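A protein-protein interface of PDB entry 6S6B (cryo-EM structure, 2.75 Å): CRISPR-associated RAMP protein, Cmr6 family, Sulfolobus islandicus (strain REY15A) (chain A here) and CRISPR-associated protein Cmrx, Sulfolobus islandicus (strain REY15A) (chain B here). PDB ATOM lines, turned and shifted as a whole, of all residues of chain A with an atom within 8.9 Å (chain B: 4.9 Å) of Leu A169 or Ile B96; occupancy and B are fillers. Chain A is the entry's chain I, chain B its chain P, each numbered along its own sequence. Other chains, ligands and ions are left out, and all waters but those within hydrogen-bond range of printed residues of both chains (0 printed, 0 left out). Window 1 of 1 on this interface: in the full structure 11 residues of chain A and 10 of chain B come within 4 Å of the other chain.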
ATOM      1  N   VAL A 161      29.484 -16.720  16.449  1.00  0.00           N
ATOM      2  CA  VAL A 161      28.481 -16.161  15.550  1.00  0.00           C
ATOM      3  C   VAL A 161      28.549 -14.642  15.551  1.00  0.00           C
ATOM      4  O   VAL A 161      28.455 -13.999  14.500  1.00  0.00           O
ATOM      5  CB  VAL A 161      27.081 -16.659  15.946  1.00  0.00           C
ATOM      6  CG1 VAL A 161      26.010 -15.820  15.285  1.00  0.00           C
ATOM      7  CG2 VAL A 161      26.922 -18.116  15.581  1.00  0.00           C
ATOM      8  N   ARG A 162      28.714 -14.043  16.731  1.00  0.00           N
ATOM      9  CA  ARG A 162      28.733 -12.588  16.825  1.00  0.00           C
ATOM     10  C   ARG A 162      29.931 -12.002  16.096  1.00  0.00           C
ATOM     11  O   ARG A 162      29.817 -10.954  15.454  1.00  0.00           O
ATOM     12  CB  ARG A 162      28.739 -12.158  18.285  1.00  0.00           C
ATOM     13  CG  ARG A 162      28.771 -10.666  18.477  1.00  0.00           C
ATOM     14  CD  ARG A 162      29.034 -10.309  19.917  1.00  0.00           C
ATOM     15  NE  ARG A 162      29.502  -8.937  20.044  1.00  0.00           N
ATOM     16  CZ  ARG A 162      28.767  -7.943  20.522  1.00  0.00           C
ATOM     17  NH1 ARG A 162      27.528  -8.166  20.924  1.00  0.00           N
ATOM     18  NH2 ARG A 162      29.272  -6.723  20.602  1.00  0.00           N
ATOM     19  N   SER A 163      31.088 -12.660  16.179  1.00  0.00           N
ATOM     20  CA  SER A 163      32.260 -12.155  15.475  1.00  0.00           C
ATOM     21  C   SER A 163      32.068 -12.201  13.969  1.00  0.00           C
ATOM     22  O   SER A 163      32.691 -11.421  13.242  1.00  0.00           O
ATOM     23  CB  SER A 163      33.498 -12.952  15.866  1.00  0.00           C
ATOM     24  OG  SER A 163      33.546 -14.172  15.155  1.00  0.00           O
ATOM     25  N   TYR A 164      31.217 -13.100  13.479  1.00  0.00           N
ATOM     26  CA  TYR A 164      30.970 -13.159  12.046  1.00  0.00           C
ATOM     27  C   TYR A 164      29.970 -12.109  11.598  1.00  0.00           C
ATOM     28  O   TYR A 164      30.094 -11.577  10.494  1.00  0.00           O
ATOM     29  CB  TYR A 164      30.470 -14.538  11.638  1.00  0.00           C
ATOM     30  CG  TYR A 164      29.916 -14.559  10.237  1.00  0.00           C
ATOM     31  CD1 TYR A 164      30.759 -14.557   9.139  1.00  0.00           C
ATOM     32  CD2 TYR A 164      28.550 -14.555  10.011  1.00  0.00           C
ATOM     33  CE1 TYR A 164      30.256 -14.567   7.858  1.00  0.00           C
ATOM     34  CE2 TYR A 164      28.040 -14.561   8.734  1.00  0.00           C
ATOM     35  CZ  TYR A 164      28.894 -14.566   7.662  1.00  0.00           C
ATOM     36  OH  TYR A 164      28.379 -14.573   6.390  1.00  0.00           O
ATOM     37  N   ILE A 165      28.972 -11.807  12.421  1.00  0.00           N
ATOM     38  CA  ILE A 165      28.037 -10.747  12.067  1.00  0.00           C
ATOM     39  C   ILE A 165      28.675  -9.384  12.270  1.00  0.00           C
ATOM     40  O   ILE A 165      28.503  -8.478  11.449  1.00  0.00           O
ATOM     41  CB  ILE A 165      26.738 -10.896  12.874  1.00  0.00           C
ATOM     42  CG1 ILE A 165      25.825 -11.921  12.211  1.00  0.00           C
ATOM     43  CG2 ILE A 165      26.039  -9.565  13.009  1.00  0.00           C
ATOM     44  CD1 ILE A 165      24.551 -12.167  12.964  1.00  0.00           C
ATOM     45  N   GLU A 166      29.428  -9.215  13.358  1.00  0.00           N
ATOM     46  CA  GLU A 166      30.120  -7.953  13.580  1.00  0.00           C
ATOM     47  C   GLU A 166      31.134  -7.680  12.482  1.00  0.00           C
ATOM     48  O   GLU A 166      31.388  -6.518  12.145  1.00  0.00           O
ATOM     49  CB  GLU A 166      30.802  -7.956  14.946  1.00  0.00           C
ATOM     50  CG  GLU A 166      31.493  -6.651  15.286  1.00  0.00           C
ATOM     51  CD  GLU A 166      32.609  -6.814  16.299  1.00  0.00           C
ATOM     52  OE1 GLU A 166      32.433  -7.593  17.260  1.00  0.00           O
ATOM     53  OE2 GLU A 166      33.660  -6.157  16.138  1.00  0.00           O
ATOM     54  N   GLY A 167      31.714  -8.725  11.907  1.00  0.00           N
ATOM     55  CA  GLY A 167      32.634  -8.556  10.804  1.00  0.00           C
ATOM     56  C   GLY A 167      31.920  -8.331   9.489  1.00  0.00           C
ATOM     57  O   GLY A 167      32.364  -7.528   8.666  1.00  0.00           O
ATOM     58  N   LYS A 168      30.810  -9.037   9.281  1.00  0.00           N
ATOM     59  CA  LYS A 168      30.058  -8.898   8.039  1.00  0.00           C
ATOM     60  C   LYS A 168      29.124  -7.695   8.081  1.00  0.00           C
ATOM     61  O   LYS A 168      29.249  -6.771   7.273  1.00  0.00           O
ATOM     62  CB  LYS A 168      29.264 -10.173   7.759  1.00  0.00           C
ATOM     63  CG  LYS A 168      28.129  -9.981   6.776  1.00  0.00           C
ATOM     64  CD  LYS A 168      27.097 -11.082   6.891  1.00  0.00           C
ATOM     65  CE  LYS A 168      26.152 -11.060   5.703  1.00  0.00           C
ATOM     66  NZ  LYS A 168      25.038 -12.036   5.838  1.00  0.00           N
ATOM     67  N   LEU A 169      28.180  -7.686   9.020  1.00  0.00           N
ATOM     68  CA  LEU A 169      27.127  -6.683   9.059  1.00  0.00           C
ATOM     69  C   LEU A 169      27.509  -5.448   9.859  1.00  0.00           C
ATOM     70  O   LEU A 169      26.626  -4.674  10.241  1.00  0.00           O
ATOM     71  CB  LEU A 169      25.843  -7.289   9.627  1.00  0.00           C
ATOM     72  CG  LEU A 169      25.153  -8.351   8.771  1.00  0.00           C
ATOM     73  CD1 LEU A 169      23.745  -8.598   9.268  1.00  0.00           C
ATOM     74  CD2 LEU A 169      25.135  -7.933   7.318  1.00  0.00           C
ATOM     75  N   GLY A 170      28.787  -5.245  10.119  1.00  0.00           N
ATOM     76  CA  GLY A 170      29.209  -4.066  10.836  1.00  0.00           C
ATOM     77  C   GLY A 170      28.983  -4.179  12.330  1.00  0.00           C
ATOM     78  O   GLY A 170      28.675  -5.237  12.875  1.00  0.00           O
ATOM     79  N   GLU A 171      29.130  -3.039  12.998  1.00  0.00           N
ATOM     80  CA  GLU A 171      29.073  -2.984  14.451  1.00  0.00           C
ATOM     81  C   GLU A 171      27.664  -2.718  14.966  1.00  0.00           C
ATOM     82  O   GLU A 171      27.176  -3.437  15.840  1.00  0.00           O
ATOM     83  CB  GLU A 171      30.026  -1.905  14.964  1.00  0.00           C
ATOM     84  CG  GLU A 171      30.130  -1.830  16.471  1.00  0.00           C
ATOM     85  CD  GLU A 171      31.072  -2.867  17.035  1.00  0.00           C
ATOM     86  OE1 GLU A 171      31.692  -3.603  16.242  1.00  0.00           O
ATOM     87  OE2 GLU A 171      31.195  -2.944  18.275  1.00  0.00           O
ATOM     88  N   GLN A 172      27.004  -1.689  14.436  1.00  0.00           N
ATOM     89  CA  GLN A 172      25.692  -1.306  14.945  1.00  0.00           C
ATOM     90  C   GLN A 172      24.652  -2.392  14.721  1.00  0.00           C
ATOM     91  O   GLN A 172      23.680  -2.480  15.478  1.00  0.00           O
ATOM     92  CB  GLN A 172      25.240   0.003  14.301  1.00  0.00           C
ATOM     93  CG  GLN A 172      25.873   1.239  14.908  1.00  0.00           C
ATOM     94  CD  GLN A 172      27.367   1.304  14.688  1.00  0.00           C
ATOM     95  OE1 GLN A 172      28.142   1.328  15.641  1.00  0.00           O
ATOM     96  NE2 GLN A 172      27.782   1.327  13.428  1.00  0.00           N
ATOM     97  N   GLU A 173      24.825  -3.223  13.694  1.00  0.00           N
ATOM     98  CA  GLU A 173      23.882  -4.315  13.493  1.00  0.00           C
ATOM     99  C   GLU A 173      24.106  -5.424  14.507  1.00  0.00           C
ATOM    100  O   GLU A 173      23.145  -6.038  14.983  1.00  0.00           O
ATOM    101  CB  GLU A 173      23.986  -4.859  12.073  1.00  0.00           C
ATOM    102  CG  GLU A 173      23.021  -6.001  11.783  1.00  0.00           C
ATOM    103  CD  GLU A 173      21.559  -5.575  11.838  1.00  0.00           C
ATOM    104  OE1 GLU A 173      21.281  -4.368  11.678  1.00  0.00           O
ATOM    105  OE2 GLU A 173      20.687  -6.447  12.032  1.00  0.00           O
ATOM    106  N   ALA A 174      25.363  -5.695  14.856  1.00  0.00           N
ATOM    107  CA  ALA A 174      25.647  -6.705  15.867  1.00  0.00           C
ATOM    108  C   ALA A 174      25.082  -6.290  17.217  1.00  0.00           C
ATOM    109  O   ALA A 174      24.264  -7.001  17.810  1.00  0.00           O
ATOM    110  CB  ALA A 174      27.153  -6.947  15.959  1.00  0.00           C
ATOM    111  N   GLU A 175      25.487  -5.121  17.708  1.00  0.00           N
ATOM    112  CA  GLU A 175      24.999  -4.634  18.990  1.00  0.00           C
ATOM    113  C   GLU A 175      23.507  -4.365  18.993  1.00  0.00           C
ATOM    114  O   GLU A 175      22.968  -3.996  20.040  1.00  0.00           O
ATOM    115  CB  GLU A 175      25.756  -3.373  19.393  1.00  0.00           C
ATOM    116  CG  GLU A 175      27.261  -3.544  19.376  1.00  0.00           C
ATOM    117  CD  GLU A 175      27.970  -2.528  20.242  1.00  0.00           C
ATOM    118  OE1 GLU A 175      27.280  -1.690  20.857  1.00  0.00           O
ATOM    119  OE2 GLU A 175      29.217  -2.570  20.311  1.00  0.00           O
ATOM    120  N   GLU A 176      22.830  -4.531  17.861  1.00  0.00           N
ATOM    121  CA  GLU A 176      21.378  -4.513  17.817  1.00  0.00           C
ATOM    122  C   GLU A 176      20.781  -5.910  17.860  1.00  0.00           C
ATOM    123  O   GLU A 176      19.562  -6.041  17.989  1.00  0.00           O
ATOM    124  CB  GLU A 176      20.890  -3.788  16.560  1.00  0.00           C
ATOM    125  CG  GLU A 176      19.523  -3.146  16.710  1.00  0.00           C
ATOM    126  CD  GLU A 176      19.501  -2.066  17.772  1.00  0.00           C
ATOM    127  OE1 GLU A 176      20.486  -1.306  17.866  1.00  0.00           O
ATOM    128  OE2 GLU A 176      18.502  -1.977  18.516  1.00  0.00           O
ATOM    129  N   ILE A 177      21.608  -6.946  17.748  1.00  0.00           N
ATOM    130  CA  ILE A 177      21.162  -8.321  17.883  1.00  0.00           C
ATOM    131  C   ILE A 177      21.703  -8.961  19.154  1.00  0.00           C
ATOM    132  O   ILE A 177      20.999  -9.727  19.813  1.00  0.00           O
ATOM    133  CB  ILE A 177      21.552  -9.153  16.644  1.00  0.00           C
ATOM    134  CG1 ILE A 177      21.161  -8.423  15.370  1.00  0.00           C
ATOM    135  CG2 ILE A 177      20.865 -10.493  16.668  1.00  0.00           C
ATOM    136  CD1 ILE A 177      21.556  -9.160  14.131  1.00  0.00           C
ATOM    137  N   PHE A 178      22.941  -8.653  19.519  1.00  0.00           N
ATOM    138  CA  PHE A 178      23.561  -9.223  20.701  1.00  0.00           C
ATOM    139  C   PHE A 178      23.735  -8.221  21.830  1.00  0.00           C
ATOM    140  O   PHE A 178      24.252  -8.588  22.887  1.00  0.00           O
ATOM    141  CB  PHE A 178      24.916  -9.830  20.339  1.00  0.00           C
ATOM    142  CG  PHE A 178      24.854 -10.817  19.220  1.00  0.00           C
ATOM    143  CD1 PHE A 178      24.574 -12.143  19.470  1.00  0.00           C
ATOM    144  CD2 PHE A 178      25.083 -10.423  17.921  1.00  0.00           C
ATOM    145  CE1 PHE A 178      24.518 -13.051  18.449  1.00  0.00           C
ATOM    146  CE2 PHE A 178      25.028 -11.332  16.897  1.00  0.00           C
ATOM    147  CZ  PHE A 178      24.745 -12.647  17.163  1.00  0.00           C
ATOM    148  N   ASP A 246      12.743  -9.979  13.916  1.00  0.00           N
ATOM    149  CA  ASP A 246      13.811  -9.105  13.448  1.00  0.00           C
ATOM    150  C   ASP A 246      15.162  -9.810  13.397  1.00  0.00           C
ATOM    151  O   ASP A 246      15.944  -9.593  12.469  1.00  0.00           O
ATOM    152  CB  ASP A 246      13.889  -7.878  14.359  1.00  0.00           C
ATOM    153  CG  ASP A 246      14.644  -6.728  13.735  1.00  0.00           C
ATOM    154  OD1 ASP A 246      15.226  -6.908  12.646  1.00  0.00           O
ATOM    155  OD2 ASP A 246      14.652  -5.637  14.340  1.00  0.00           O
ATOM    156  N   LYS A 249      16.398 -13.722  10.695  1.00  0.00           N
ATOM    157  CA  LYS A 249      17.104 -13.887   9.425  1.00  0.00           C
ATOM    158  C   LYS A 249      18.618 -13.915   9.594  1.00  0.00           C
ATOM    159  O   LYS A 249      19.254 -14.850   9.077  1.00  0.00           O
ATOM    160  CB  LYS A 249      16.667 -12.800   8.440  1.00  0.00           C
ATOM    161  CG  LYS A 249      15.176 -12.758   8.199  1.00  0.00           C
ATOM    162  CD  LYS A 249      14.685 -14.094   7.676  1.00  0.00           C
ATOM    163  CE  LYS A 249      13.173 -14.142   7.584  1.00  0.00           C
ATOM    164  NZ  LYS A 249      12.685 -15.518   7.303  1.00  0.00           N
ATOM    165  N   PRO A 250      19.259 -12.957  10.274  1.00  0.00           N
ATOM    166  CA  PRO A 250      20.730 -12.954  10.314  1.00  0.00           C
ATOM    167  C   PRO A 250      21.341 -14.145  11.023  1.00  0.00           C
ATOM    168  O   PRO A 250      22.549 -14.366  10.882  1.00  0.00           O
ATOM    169  CB  PRO A 250      21.057 -11.652  11.052  1.00  0.00           C
ATOM    170  CG  PRO A 250      19.848 -11.358  11.836  1.00  0.00           C
ATOM    171  CD  PRO A 250      18.708 -11.797  10.995  1.00  0.00           C
ATOM    172  N   ILE A 251      20.567 -14.913  11.776  1.00  0.00           N
ATOM    173  CA  ILE A 251      21.093 -16.106  12.427  1.00  0.00           C
ATOM    174  C   ILE A 251      20.991 -17.316  11.517  1.00  0.00           C
ATOM    175  O   ILE A 251      21.966 -18.047  11.328  1.00  0.00           O
ATOM    176  CB  ILE A 251      20.363 -16.342  13.762  1.00  0.00           C
ATOM    177  CG1 ILE A 251      20.504 -15.116  14.660  1.00  0.00           C
ATOM    178  CG2 ILE A 251      20.922 -17.566  14.454  1.00  0.00           C
ATOM    179  CD1 ILE A 251      21.899 -14.924  15.198  1.00  0.00           C
ATOM    180  N   ASP A 253      20.899 -17.166   8.451  1.00  0.00           N
ATOM    181  CA  ASP A 253      21.859 -16.896   7.390  1.00  0.00           C
ATOM    182  C   ASP A 253      23.272 -17.269   7.811  1.00  0.00           C
ATOM    183  O   ASP A 253      23.967 -18.008   7.107  1.00  0.00           O
ATOM    184  CB  ASP A 253      21.802 -15.422   7.003  1.00  0.00           C
ATOM    185  CG  ASP A 253      22.826 -15.063   5.954  1.00  0.00           C
ATOM    186  OD1 ASP A 253      22.635 -15.433   4.777  1.00  0.00           O
ATOM    187  OD2 ASP A 253      23.830 -14.415   6.311  1.00  0.00           O
ATOM    188  N   SER A 254      23.716 -16.758   8.957  1.00  0.00           N
ATOM    189  CA  SER A 254      25.122 -16.854   9.319  1.00  0.00           C
ATOM    190  C   SER A 254      25.540 -18.281   9.633  1.00  0.00           C
ATOM    191  O   SER A 254      26.680 -18.662   9.348  1.00  0.00           O
ATOM    192  CB  SER A 254      25.405 -15.955  10.517  1.00  0.00           C
ATOM    193  OG  SER A 254      24.733 -16.437  11.662  1.00  0.00           O
ATOM    194  N   HIS B  39      18.900   2.931   7.423  1.00  0.00           N
ATOM    195  CA  HIS B  39      18.089   1.866   7.987  1.00  0.00           C
ATOM    196  C   HIS B  39      17.525   1.018   6.858  1.00  0.00           C
ATOM    197  O   HIS B  39      17.582   1.394   5.687  1.00  0.00           O
ATOM    198  CB  HIS B  39      16.955   2.429   8.850  1.00  0.00           C
ATOM    199  CG  HIS B  39      17.365   3.577   9.718  1.00  0.00           C
ATOM    200  ND1 HIS B  39      18.365   3.478  10.662  1.00  0.00           N
ATOM    201  CD2 HIS B  39      16.909   4.849   9.787  1.00  0.00           C
ATOM    202  CE1 HIS B  39      18.507   4.639  11.274  1.00  0.00           C
ATOM    203  NE2 HIS B  39      17.635   5.488  10.762  1.00  0.00           N
ATOM    204  N   ASN B  40      16.979  -0.139   7.227  1.00  0.00           N
ATOM    205  CA  ASN B  40      16.278  -1.035   6.306  1.00  0.00           C
ATOM    206  C   ASN B  40      17.114  -1.339   5.065  1.00  0.00           C
ATOM    207  O   ASN B  40      16.744  -1.019   3.936  1.00  0.00           O
ATOM    208  CB  ASN B  40      14.921  -0.451   5.914  1.00  0.00           C
ATOM    209  CG  ASN B  40      14.078  -0.084   7.110  1.00  0.00           C
ATOM    210  OD1 ASN B  40      13.353  -0.917   7.648  1.00  0.00           O
ATOM    211  ND2 ASN B  40      14.161   1.171   7.527  1.00  0.00           N
ATOM    212  N   VAL B  41      18.258  -1.971   5.292  1.00  0.00           N
ATOM    213  CA  VAL B  41      19.157  -2.376   4.218  1.00  0.00           C
ATOM    214  C   VAL B  41      18.925  -3.852   3.935  1.00  0.00           C
ATOM    215  O   VAL B  41      19.035  -4.690   4.838  1.00  0.00           O
ATOM    216  CB  VAL B  41      20.625  -2.110   4.584  1.00  0.00           C
ATOM    217  CG1 VAL B  41      21.543  -2.789   3.589  1.00  0.00           C
ATOM    218  CG2 VAL B  41      20.897  -0.620   4.636  1.00  0.00           C
ATOM    219  N   VAL B  43      20.007  -7.401   2.428  1.00  0.00           N
ATOM    220  CA  VAL B  43      21.271  -8.110   2.229  1.00  0.00           C
ATOM    221  C   VAL B  43      20.928  -9.416   1.522  1.00  0.00           C
ATOM    222  O   VAL B  43      20.592 -10.421   2.154  1.00  0.00           O
ATOM    223  CB  VAL B  43      22.013  -8.362   3.543  1.00  0.00           C
ATOM    224  CG1 VAL B  43      23.261  -9.190   3.300  1.00  0.00           C
ATOM    225  CG2 VAL B  43      22.360  -7.051   4.222  1.00  0.00           C
ATOM    226  N   LYS B  67      24.596  -5.888  -0.480  1.00  0.00           N
ATOM    227  CA  LYS B  67      23.698  -5.037   0.286  1.00  0.00           C
ATOM    228  C   LYS B  67      23.357  -3.795  -0.524  1.00  0.00           C
ATOM    229  O   LYS B  67      24.237  -3.195  -1.150  1.00  0.00           O
ATOM    230  CB  LYS B  67      24.327  -4.650   1.624  1.00  0.00           C
ATOM    231  CG  LYS B  67      25.213  -5.731   2.210  1.00  0.00           C
ATOM    232  CD  LYS B  67      25.562  -5.429   3.650  1.00  0.00           C
ATOM    233  CE  LYS B  67      26.859  -6.101   4.054  1.00  0.00           C
ATOM    234  NZ  LYS B  67      27.131  -5.933   5.504  1.00  0.00           N
ATOM    235  N   TYR B  94      15.600  -9.616   4.390  1.00  0.00           N
ATOM    236  CA  TYR B  94      16.791  -9.519   5.231  1.00  0.00           C
ATOM    237  C   TYR B  94      17.142  -8.042   5.417  1.00  0.00           C
ATOM    238  O   TYR B  94      18.146  -7.531   4.920  1.00  0.00           O
ATOM    239  CB  TYR B  94      17.936 -10.294   4.598  1.00  0.00           C
ATOM    240  CG  TYR B  94      19.082 -10.633   5.520  1.00  0.00           C
ATOM    241  CD1 TYR B  94      19.301 -11.934   5.937  1.00  0.00           C
ATOM    242  CD2 TYR B  94      19.952  -9.654   5.964  1.00  0.00           C
ATOM    243  CE1 TYR B  94      20.356 -12.248   6.764  1.00  0.00           C
ATOM    244  CE2 TYR B  94      21.005  -9.957   6.793  1.00  0.00           C
ATOM    245  CZ  TYR B  94      21.203 -11.252   7.190  1.00  0.00           C
ATOM    246  OH  TYR B  94      22.263 -11.539   8.017  1.00  0.00           O
ATOM    247  N   LEU B  95      16.271  -7.344   6.138  1.00  0.00           N
ATOM    248  CA  LEU B  95      16.487  -5.934   6.433  1.00  0.00           C
ATOM    249  C   LEU B  95      17.333  -5.809   7.692  1.00  0.00           C
ATOM    250  O   LEU B  95      16.961  -6.329   8.748  1.00  0.00           O
ATOM    251  CB  LEU B  95      15.156  -5.209   6.608  1.00  0.00           C
ATOM    252  CG  LEU B  95      14.221  -5.145   5.400  1.00  0.00           C
ATOM    253  CD1 LEU B  95      12.781  -4.978   5.844  1.00  0.00           C
ATOM    254  CD2 LEU B  95      14.627  -4.020   4.464  1.00  0.00           C
ATOM    255  N   ILE B  96      18.468  -5.130   7.583  1.00  0.00           N
ATOM    256  CA  ILE B  96      19.318  -4.866   8.731  1.00  0.00           C
ATOM    257  C   ILE B  96      19.178  -3.398   9.101  1.00  0.00           C
ATOM    258  O   ILE B  96      18.722  -2.568   8.309  1.00  0.00           O
ATOM    259  CB  ILE B  96      20.792  -5.232   8.476  1.00  0.00           C
ATOM    260  CG1 ILE B  96      21.403  -4.320   7.417  1.00  0.00           C
ATOM    261  CG2 ILE B  96      20.903  -6.672   8.039  1.00  0.00           C
ATOM    262  CD1 ILE B  96      22.902  -4.461   7.306  1.00  0.00           C
ATOM    263  N   ARG B  97      19.582  -3.081  10.331  1.00  0.00           N
ATOM    264  CA  ARG B  97      19.376  -1.757  10.910  1.00  0.00           C
ATOM    265  C   ARG B  97      17.916  -1.339  10.770  1.00  0.00           C
ATOM    266  O   ARG B  97      17.596  -0.218  10.378  1.00  0.00           O
ATOM    267  CB  ARG B  97      20.310  -0.730  10.276  1.00  0.00           C
ATOM    268  CG  ARG B  97      21.671  -0.641  10.931  1.00  0.00           C
ATOM    269  CD  ARG B  97      22.205   0.772  10.836  1.00  0.00           C
ATOM    270  NE  ARG B  97      23.591   0.880  11.274  1.00  0.00           N
ATOM    271  CZ  ARG B  97      24.283   2.015  11.273  1.00  0.00           C
ATOM    272  NH1 ARG B  97      23.715   3.139  10.856  1.00  0.00           N
ATOM    273  NH2 ARG B  97      25.539   2.028  11.688  1.00  0.00           N
ATOM    274  N   LYS B  98      17.024  -2.267  11.110  1.00  0.00           N
ATOM    275  CA  LYS B  98      15.606  -2.101  10.842  1.00  0.00           C
ATOM    276  C   LYS B  98      15.020  -0.911  11.594  1.00  0.00           C
ATOM    277  O   LYS B  98      15.571  -0.419  12.581  1.00  0.00           O
ATOM    278  CB  LYS B  98      14.840  -3.365  11.221  1.00  0.00           C
ATOM    279  CG  LYS B  98      14.801  -4.413  10.134  1.00  0.00           C
ATOM    280  CD  LYS B  98      13.644  -5.368  10.337  1.00  0.00           C
ATOM    281  CE  LYS B  98      12.354  -4.617  10.608  1.00  0.00           C
ATOM    282  NZ  LYS B  98      11.984  -3.733   9.472  1.00  0.00           N
ATOM    283  N   LEU B 166      29.159  -0.512   6.372  1.00  0.00           N
ATOM    284  CA  LEU B 166      27.959  -1.332   6.276  1.00  0.00           C
ATOM    285  C   LEU B 166      27.767  -1.968   4.910  1.00  0.00           C
ATOM    286  O   LEU B 166      27.296  -3.101   4.831  1.00  0.00           O
ATOM    287  CB  LEU B 166      26.724  -0.491   6.619  1.00  0.00           C
ATOM    288  CG  LEU B 166      25.442  -1.211   7.038  1.00  0.00           C
ATOM    289  CD1 LEU B 166      24.664  -0.357   8.021  1.00  0.00           C
ATOM    290  CD2 LEU B 166      24.584  -1.541   5.829  1.00  0.00           C
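The backbone carbonyl oxygen (O) of Lys A168 is in hydrogen-bond range of the side-chain amino group (NZ) of Lys B67 (2.9 Å).
NE2 of Gln A172 sits close to NH2 of Arg B97.
OE1 of Glu A173 is in hydrogen-bond range of N of Arg B97.
OD2 of Asp A253 lies within salt-bridge range of NZ of Lys A168, 2.7 Å away.
The backbone carbonyl oxygen of Pro A250 is in hydrogen-bond range of the side-chain hydroxyl of Ser A254 (3.1 Å).
The backbone NH (N) of Asn B40 lies within hydrogen-bond range of the backbone carbonyl oxygen (O) of Ile B96, 3.2 Å away.
O of Val B41 lies within hydrogen-bond range of N of Ile B96, 2.8 Å away.
The backbone carbonyl oxygen (O) of Tyr B94 lies within hydrogen-bond range of the backbone NH (N) of Val B43 (3.1 Å).
The backbone carbonyl oxygen (O) of Leu B166 lies within hydrogen-bond range of the side-chain amino group (NZ) of Lys B67.
NZ of Lys A168 touches OH of Tyr B94 (3.6 Å).
Leu A169 touches Lys B67 (CD2 to NZ, 3.4 Å).
OH of Tyr B94 touches CD1 of Leu A169, at 3.5 Å.
Leu A169 touches Ile B96 (CD1 to CG2, 3.6 Å).
Glu A173 touches Ile B96.
Asp A246 touches Lys B98.
CE1 of Tyr B94 touches O of Lys A249 (3.7 Å).
Tyr B94 touches Pro A250.
CB of Asp A253 touches CE1 of Tyr B94, 3.5 Å away.
Printed residues of chain B within 4 Å of Lys A168: Lys B67 and Tyr B94.
Of chain B, only Lys B67 (3.4 Å), Tyr B94 (3.5 Å) and Ile B96 (3.6 Å) come within 4 Å of Leu A169.
Printed residues of chain B within 4 Å of Glu A173: Ile B96 (3.4 Å) and Arg B97 (2.5 Å).
Printed residues of chain B within 4 Å of Pro A250: Tyr B94.
No residue of chain A comes within 4 Å of Val B41.
Printed residues of chain A within 4 Å of Lys B67: Lys A168 (2.9 Å) and Leu A169 (3.4 Å).
Ile B96 touches just these residues of chain A: Leu A169 and Glu A173.
The nearest residue of chain B that does not touch Leu A169 is Val B43 (4.3 Å).
Printed residues of chain B that touch a printed residue of chain A: Lys B67, Tyr B94, Ile B96, Arg B97 and Lys B98.
Hydrophobic or aromatic side chains of chain B that line the printed part of chain A: Tyr B94 and Ile B96.
Hydrophobic or aromatic side chains of chain A that line the printed part of chain B: Leu A169 and Pro A250.
Among the printed residues, no Asp or Glu carboxylate lies within 4 Å of a Lys or Arg side-chain nitrogen of the other chain.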
